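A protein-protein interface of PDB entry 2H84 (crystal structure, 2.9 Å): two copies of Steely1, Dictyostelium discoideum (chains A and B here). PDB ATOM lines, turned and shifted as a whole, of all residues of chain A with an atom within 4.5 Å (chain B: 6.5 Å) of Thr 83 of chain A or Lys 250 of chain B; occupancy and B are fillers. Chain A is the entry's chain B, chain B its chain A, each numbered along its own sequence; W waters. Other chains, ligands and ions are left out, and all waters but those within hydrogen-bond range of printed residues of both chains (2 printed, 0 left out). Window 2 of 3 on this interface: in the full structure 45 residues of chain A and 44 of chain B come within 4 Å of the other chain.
Of the printed residues of chain A, Lys 250 of chain B touches Thr 83 (3.6 Å), Ile 84 (3.4 Å) and Thr 85 (2.8 Å). Of the printed residues of chain B, Thr 85 of chain A touches Glu 249 and Lys 250. Printed residues of chain A within 4 Å of Leu 248 of chain B: Ile 84 (3.6 Å). Of the printed residues of chain B, Lys 250 of chain A touches Thr 83, Ile 84 and Thr 85. Printed residues of chain A within 4 Å of Thr 85 of chain B: Lys 250 (2.8 Å). Of the printed residues of chain A, Glu 249 of chain B touches Ile 84 and Thr 85. Glu 251 of chain B touches none of the printed residues of chain A. Glu 82 of chain B touches none of the printed residues of chain A. The nearest printed residue of chain A that does not touch Lys 250 of chain B is Lys 250 of chain A (4.01 Å).
Water W2 lies within hydrogen-bond range of NZ of Lys 250 of chain B (2.6 Å), OG1 of Thr 85 of chain A (2.6 Å) and OE2 of Glu 251 of chain B (2.8 Å). Water W1 lies within hydrogen-bond range of NZ of Lys 250 of chain B (2.7 Å) and OG1 of Thr 83 of chain A (3.3 Å).
The backbone NH (N) of Thr 83 of chain A lies within hydrogen-bond range of the side-chain carboxylate (OD1) of Asp 86 of chain A (2.7 Å). NZ of Lys 250 of chain A is in salt-bridge range of OE1 of Glu 251 of chain A (3.1 Å). OG1 of Thr 83 of chain B sits close to N of Thr 85 of chain B (3.3 Å). The backbone NH (N) of Ile 84 of chain B lies within hydrogen-bond range of the backbone carbonyl oxygen (O) of Lys 250 of chain B. The backbone carbonyl oxygen (O) of Lys 250 of chain A sits at hydrogen-bond distance from the backbone NH (N) of Ile 84 of chain A (2.8 Å). NZ of Lys 250 of chain B is in salt-bridge range of OE1 of Glu 251 of chain B, 2.8 Å away.
Among the printed residues, merely in contact across the chains: Thr 83 of chain A with Lys 250 of chain B, Ile 84 of chain A with Ile 84 of chain B, Ile 84 of chain A with Leu 248 of chain B, Ile 84 of chain A with Glu 249 of chain B, Ile 84 of chain A with Lys 250 of chain B, Thr 85 of chain A with Glu 249 of chain B, Lys 250 of chain A with Thr 83 of chain B and Lys 250 of chain A with Ile 84 of chain B.
Thr 83 of chain A touches Lys 250 of chain B, and with the chains exchanged Lys 250 of chain A touches Thr 83 of chain B. Ile 84 of chain A touches its own counterpart, Ile 84 of chain B. Ile 84 of chain A touches Lys 250 of chain B, and with the chains exchanged Lys 250 of chain A touches Ile 84 of chain B. Thr 85 of chain A touches Lys 250 of chain B, and with the chains exchanged Lys 250 of chain A touches Thr 85 of chain B. Of the 10 pairs that touch across the chains among the printed residues, 7 have their exchanged pair printed and touching as well.
Of the 9 printed residues of chain A, 4 touch a printed residue of chain B. Printed residues of chain B that touch a printed residue of chain A: Thr 83, Ile 84, Thr 85, Leu 248, Glu 249 and Lys 250. Hydrophobic or aromatic side chains of chain B within 4 Å of the printed part of chain A: Ile 84 and Leu 248. Among the printed residues, 10 pairs touch across the chains.
The backbone NH (N) of Lys 250 of chain B is in hydrogen-bond range of the side-chain hydroxyl (OG1) of Thr 85 of chain A (2.8 Å). The backbone NH (N) of Lys 250 of chain A is in hydrogen-bond range of the side-chain hydroxyl (OG1) of Thr 85 of chain B (2.8 Å).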
ATOM      1  N   LEU A  81     -35.642 -20.650 -13.666  1.00  0.00           N
ATOM      2  CA  LEU A  81     -35.299 -20.767 -12.257  1.00  0.00           C
ATOM      3  C   LEU A  81     -33.930 -21.360 -12.040  1.00  0.00           C
ATOM      4  O   LEU A  81     -33.481 -21.479 -10.898  1.00  0.00           O
ATOM      5  CB  LEU A  81     -36.329 -21.616 -11.521  1.00  0.00           C
ATOM      6  CG  LEU A  81     -37.735 -21.036 -11.387  1.00  0.00           C
ATOM      7  CD1 LEU A  81     -38.599 -22.045 -10.668  1.00  0.00           C
ATOM      8  CD2 LEU A  81     -37.701 -19.730 -10.617  1.00  0.00           C
ATOM      9  N   GLU A  82     -33.278 -21.739 -13.138  1.00  0.00           N
ATOM     10  CA  GLU A  82     -31.940 -22.319 -13.098  1.00  0.00           C
ATOM     11  C   GLU A  82     -30.892 -21.278 -13.490  1.00  0.00           C
ATOM     12  O   GLU A  82     -31.196 -20.280 -14.142  1.00  0.00           O
ATOM     13  CB  GLU A  82     -31.862 -23.504 -14.053  1.00  0.00           C
ATOM     14  CG  GLU A  82     -32.812 -24.619 -13.709  1.00  0.00           C
ATOM     15  CD  GLU A  82     -32.846 -25.712 -14.768  1.00  0.00           C
ATOM     16  OE1 GLU A  82     -33.147 -26.874 -14.420  1.00  0.00           O
ATOM     17  OE2 GLU A  82     -32.583 -25.416 -15.954  1.00  0.00           O
ATOM     18  N   THR A  83     -29.652 -21.509 -13.085  1.00  0.00           N
ATOM     19  CA  THR A  83     -28.571 -20.591 -13.403  1.00  0.00           C
ATOM     20  C   THR A  83     -27.481 -21.360 -14.145  1.00  0.00           C
ATOM     21  O   THR A  83     -27.602 -22.568 -14.387  1.00  0.00           O
ATOM     22  CB  THR A  83     -27.986 -19.966 -12.127  1.00  0.00           C
ATOM     23  OG1 THR A  83     -27.299 -20.969 -11.371  1.00  0.00           O
ATOM     24  CG2 THR A  83     -29.108 -19.376 -11.269  1.00  0.00           C
ATOM     25  N   ILE A  84     -26.418 -20.662 -14.513  1.00  0.00           N
ATOM     26  CA  ILE A  84     -25.326 -21.294 -15.229  1.00  0.00           C
ATOM     27  C   ILE A  84     -24.696 -22.395 -14.372  1.00  0.00           C
ATOM     28  O   ILE A  84     -24.145 -23.360 -14.894  1.00  0.00           O
ATOM     29  CB  ILE A  84     -24.261 -20.260 -15.596  1.00  0.00           C
ATOM     30  CG1 ILE A  84     -23.114 -20.933 -16.339  1.00  0.00           C
ATOM     31  CG2 ILE A  84     -23.752 -19.571 -14.348  1.00  0.00           C
ATOM     32  CD1 ILE A  84     -23.477 -21.390 -17.715  1.00  0.00           C
ATOM     33  N   THR A  85     -24.787 -22.252 -13.052  1.00  0.00           N
ATOM     34  CA  THR A  85     -24.222 -23.244 -12.147  1.00  0.00           C
ATOM     35  C   THR A  85     -24.966 -24.564 -12.311  1.00  0.00           C
ATOM     36  O   THR A  85     -24.354 -25.624 -12.396  1.00  0.00           O
ATOM     37  CB  THR A  85     -24.321 -22.801 -10.649  1.00  0.00           C
ATOM     38  OG1 THR A  85     -23.563 -21.603 -10.452  1.00  0.00           O
ATOM     39  CG2 THR A  85     -23.769 -23.885  -9.734  1.00  0.00           C
ATOM     40  N   ASP A  86     -26.290 -24.485 -12.353  1.00  0.00           N
ATOM     41  CA  ASP A  86     -27.129 -25.662 -12.484  1.00  0.00           C
ATOM     42  C   ASP A  86     -26.821 -26.462 -13.725  1.00  0.00           C
ATOM     43  O   ASP A  86     -26.410 -27.608 -13.654  1.00  0.00           O
ATOM     44  CB  ASP A  86     -28.595 -25.254 -12.481  1.00  0.00           C
ATOM     45  CG  ASP A  86     -28.990 -24.606 -11.183  1.00  0.00           C
ATOM     46  OD1 ASP A  86     -29.295 -23.392 -11.177  1.00  0.00           O
ATOM     47  OD2 ASP A  86     -28.975 -25.318 -10.146  1.00  0.00           O
ATOM     48  N   VAL A  87     -27.020 -25.857 -14.881  1.00  0.00           N
ATOM     49  CA  VAL A  87     -26.775 -26.546 -16.135  1.00  0.00           C
ATOM     50  C   VAL A  87     -25.323 -27.069 -16.316  1.00  0.00           C
ATOM     51  O   VAL A  87     -25.106 -28.190 -16.826  1.00  0.00           O
ATOM     52  CB  VAL A  87     -27.184 -25.624 -17.304  1.00  0.00           C
ATOM     53  CG1 VAL A  87     -28.716 -25.509 -17.366  1.00  0.00           C
ATOM     54  CG2 VAL A  87     -26.634 -24.242 -17.100  1.00  0.00           C
ATOM     55  N   LYS A 250     -24.755 -15.398 -16.134  1.00  0.00           N
ATOM     56  CA  LYS A 250     -25.242 -15.988 -14.893  1.00  0.00           C
ATOM     57  C   LYS A 250     -26.481 -16.878 -14.990  1.00  0.00           C
ATOM     58  O   LYS A 250     -26.558 -17.913 -14.315  1.00  0.00           O
ATOM     59  CB  LYS A 250     -25.458 -14.893 -13.846  1.00  0.00           C
ATOM     60  CG  LYS A 250     -26.406 -13.779 -14.226  1.00  0.00           C
ATOM     61  CD  LYS A 250     -26.533 -12.768 -13.080  1.00  0.00           C
ATOM     62  CE  LYS A 250     -27.520 -11.668 -13.437  1.00  0.00           C
ATOM     63  NZ  LYS A 250     -27.143 -11.076 -14.758  1.00  0.00           N
ATOM     64  N   GLU A 251     -27.445 -16.486 -15.814  1.00  0.00           N
ATOM     65  CA  GLU A 251     -28.670 -17.265 -15.990  1.00  0.00           C
ATOM     66  C   GLU A 251     -28.422 -18.515 -16.827  1.00  0.00           C
ATOM     67  O   GLU A 251     -29.159 -19.502 -16.732  1.00  0.00           O
ATOM     68  CB  GLU A 251     -29.749 -16.423 -16.679  1.00  0.00           C
ATOM     69  CG  GLU A 251     -30.149 -15.154 -15.950  1.00  0.00           C
ATOM     70  CD  GLU A 251     -29.197 -13.996 -16.188  1.00  0.00           C
ATOM     71  OE1 GLU A 251     -29.450 -12.913 -15.625  1.00  0.00           O
ATOM     72  OE2 GLU A 251     -28.205 -14.156 -16.934  1.00  0.00           O
ATOM     73  N   GLU B  82     -20.201  -8.986  -8.026  1.00  0.00           N
ATOM     74  CA  GLU B  82     -20.118  -9.264  -9.451  1.00  0.00           C
ATOM     75  C   GLU B  82     -20.531 -10.703  -9.717  1.00  0.00           C
ATOM     76  O   GLU B  82     -20.524 -11.527  -8.811  1.00  0.00           O
ATOM     77  CB  GLU B  82     -18.692  -9.024  -9.931  1.00  0.00           C
ATOM     78  CG  GLU B  82     -18.273  -7.577  -9.815  1.00  0.00           C
ATOM     79  CD  GLU B  82     -16.809  -7.366 -10.147  1.00  0.00           C
ATOM     80  OE1 GLU B  82     -16.486  -6.355 -10.812  1.00  0.00           O
ATOM     81  OE2 GLU B  82     -15.985  -8.214  -9.731  1.00  0.00           O
ATOM     82  N   THR B  83     -20.893 -10.998 -10.959  1.00  0.00           N
ATOM     83  CA  THR B  83     -21.308 -12.333 -11.341  1.00  0.00           C
ATOM     84  C   THR B  83     -20.461 -12.795 -12.523  1.00  0.00           C
ATOM     85  O   THR B  83     -19.628 -12.044 -13.027  1.00  0.00           O
ATOM     86  CB  THR B  83     -22.795 -12.327 -11.740  1.00  0.00           C
ATOM     87  OG1 THR B  83     -22.968 -11.585 -12.957  1.00  0.00           O
ATOM     88  CG2 THR B  83     -23.624 -11.659 -10.654  1.00  0.00           C
ATOM     89  N   ILE B  84     -20.679 -14.025 -12.971  1.00  0.00           N
ATOM     90  CA  ILE B  84     -19.925 -14.562 -14.096  1.00  0.00           C
ATOM     91  C   ILE B  84     -20.171 -13.709 -15.338  1.00  0.00           C
ATOM     92  O   ILE B  84     -19.333 -13.643 -16.230  1.00  0.00           O
ATOM     93  CB  ILE B  84     -20.336 -16.027 -14.391  1.00  0.00           C
ATOM     94  CG1 ILE B  84     -19.519 -16.593 -15.562  1.00  0.00           C
ATOM     95  CG2 ILE B  84     -21.821 -16.095 -14.690  1.00  0.00           C
ATOM     96  CD1 ILE B  84     -18.048 -16.772 -15.252  1.00  0.00           C
ATOM     97  N   THR B  85     -21.321 -13.051 -15.388  1.00  0.00           N
ATOM     98  CA  THR B  85     -21.642 -12.217 -16.535  1.00  0.00           C
ATOM     99  C   THR B  85     -20.708 -11.034 -16.553  1.00  0.00           C
ATOM    100  O   THR B  85     -20.208 -10.653 -17.611  1.00  0.00           O
ATOM    101  CB  THR B  85     -23.099 -11.673 -16.499  1.00  0.00           C
ATOM    102  OG1 THR B  85     -24.027 -12.767 -16.470  1.00  0.00           O
ATOM    103  CG2 THR B  85     -23.387 -10.820 -17.746  1.00  0.00           C
ATOM    104  N   LEU B 248     -17.054 -23.294 -13.195  1.00  0.00           N
ATOM    105  CA  LEU B 248     -17.900 -22.245 -13.746  1.00  0.00           C
ATOM    106  C   LEU B 248     -19.154 -22.153 -12.900  1.00  0.00           C
ATOM    107  O   LEU B 248     -19.925 -23.104 -12.828  1.00  0.00           O
ATOM    108  CB  LEU B 248     -18.287 -22.569 -15.190  1.00  0.00           C
ATOM    109  CG  LEU B 248     -19.317 -21.630 -15.827  1.00  0.00           C
ATOM    110  CD1 LEU B 248     -18.688 -20.285 -16.162  1.00  0.00           C
ATOM    111  CD2 LEU B 248     -19.858 -22.274 -17.085  1.00  0.00           C
ATOM    112  N   GLU B 249     -19.354 -21.013 -12.255  1.00  0.00           N
ATOM    113  CA  GLU B 249     -20.521 -20.814 -11.411  1.00  0.00           C
ATOM    114  C   GLU B 249     -21.104 -19.417 -11.629  1.00  0.00           C
ATOM    115  O   GLU B 249     -20.418 -18.516 -12.101  1.00  0.00           O
ATOM    116  CB  GLU B 249     -20.145 -21.011  -9.935  1.00  0.00           C
ATOM    117  CG  GLU B 249     -19.527 -22.369  -9.643  1.00  0.00           C
ATOM    118  CD  GLU B 249     -19.304 -22.614  -8.160  1.00  0.00           C
ATOM    119  OE1 GLU B 249     -19.030 -21.633  -7.436  1.00  0.00           O
ATOM    120  OE2 GLU B 249     -19.387 -23.783  -7.717  1.00  0.00           O
ATOM    121  N   LYS B 250     -22.374 -19.238 -11.291  1.00  0.00           N
ATOM    122  CA  LYS B 250     -23.017 -17.942 -11.474  1.00  0.00           C
ATOM    123  C   LYS B 250     -22.237 -16.770 -10.890  1.00  0.00           C
ATOM    124  O   LYS B 250     -22.186 -15.689 -11.487  1.00  0.00           O
ATOM    125  CB  LYS B 250     -24.451 -17.963 -10.908  1.00  0.00           C
ATOM    126  CG  LYS B 250     -24.565 -18.398  -9.450  1.00  0.00           C
ATOM    127  CD  LYS B 250     -26.020 -18.514  -9.014  1.00  0.00           C
ATOM    128  CE  LYS B 250     -26.116 -18.932  -7.560  1.00  0.00           C
ATOM    129  NZ  LYS B 250     -25.343 -20.161  -7.289  1.00  0.00           N
ATOM    130  N   GLU B 251     -21.639 -16.978  -9.720  1.00  0.00           N
ATOM    131  CA  GLU B 251     -20.881 -15.925  -9.042  1.00  0.00           C
ATOM    132  C   GLU B 251     -19.564 -15.590  -9.749  1.00  0.00           C
ATOM    133  O   GLU B 251     -19.002 -14.505  -9.564  1.00  0.00           O
ATOM    134  CB  GLU B 251     -20.604 -16.327  -7.586  1.00  0.00           C
ATOM    135  CG  GLU B 251     -21.846 -16.687  -6.775  1.00  0.00           C
ATOM    136  CD  GLU B 251     -22.345 -18.080  -7.043  1.00  0.00           C
ATOM    137  OE1 GLU B 251     -23.330 -18.472  -6.387  1.00  0.00           O
ATOM    138  OE2 GLU B 251     -21.747 -18.775  -7.896  1.00  0.00           O
ATOM    139  N   GLY B 252     -19.105 -16.515 -10.592  1.00  0.00           N
ATOM    140  CA  GLY B 252     -17.847 -16.362 -11.318  1.00  0.00           C
ATOM    141  C   GLY B 252     -17.092 -17.683 -11.255  1.00  0.00           C
ATOM    142  O   GLY B 252     -17.662 -18.680 -10.853  1.00  0.00           O
HETATM  143  O   HOH W   1     -27.297 -21.862  -8.210  1.00  0.00           O
HETATM  144  O   HOH W   2     -23.101 -21.259  -7.889  1.00  0.00           O
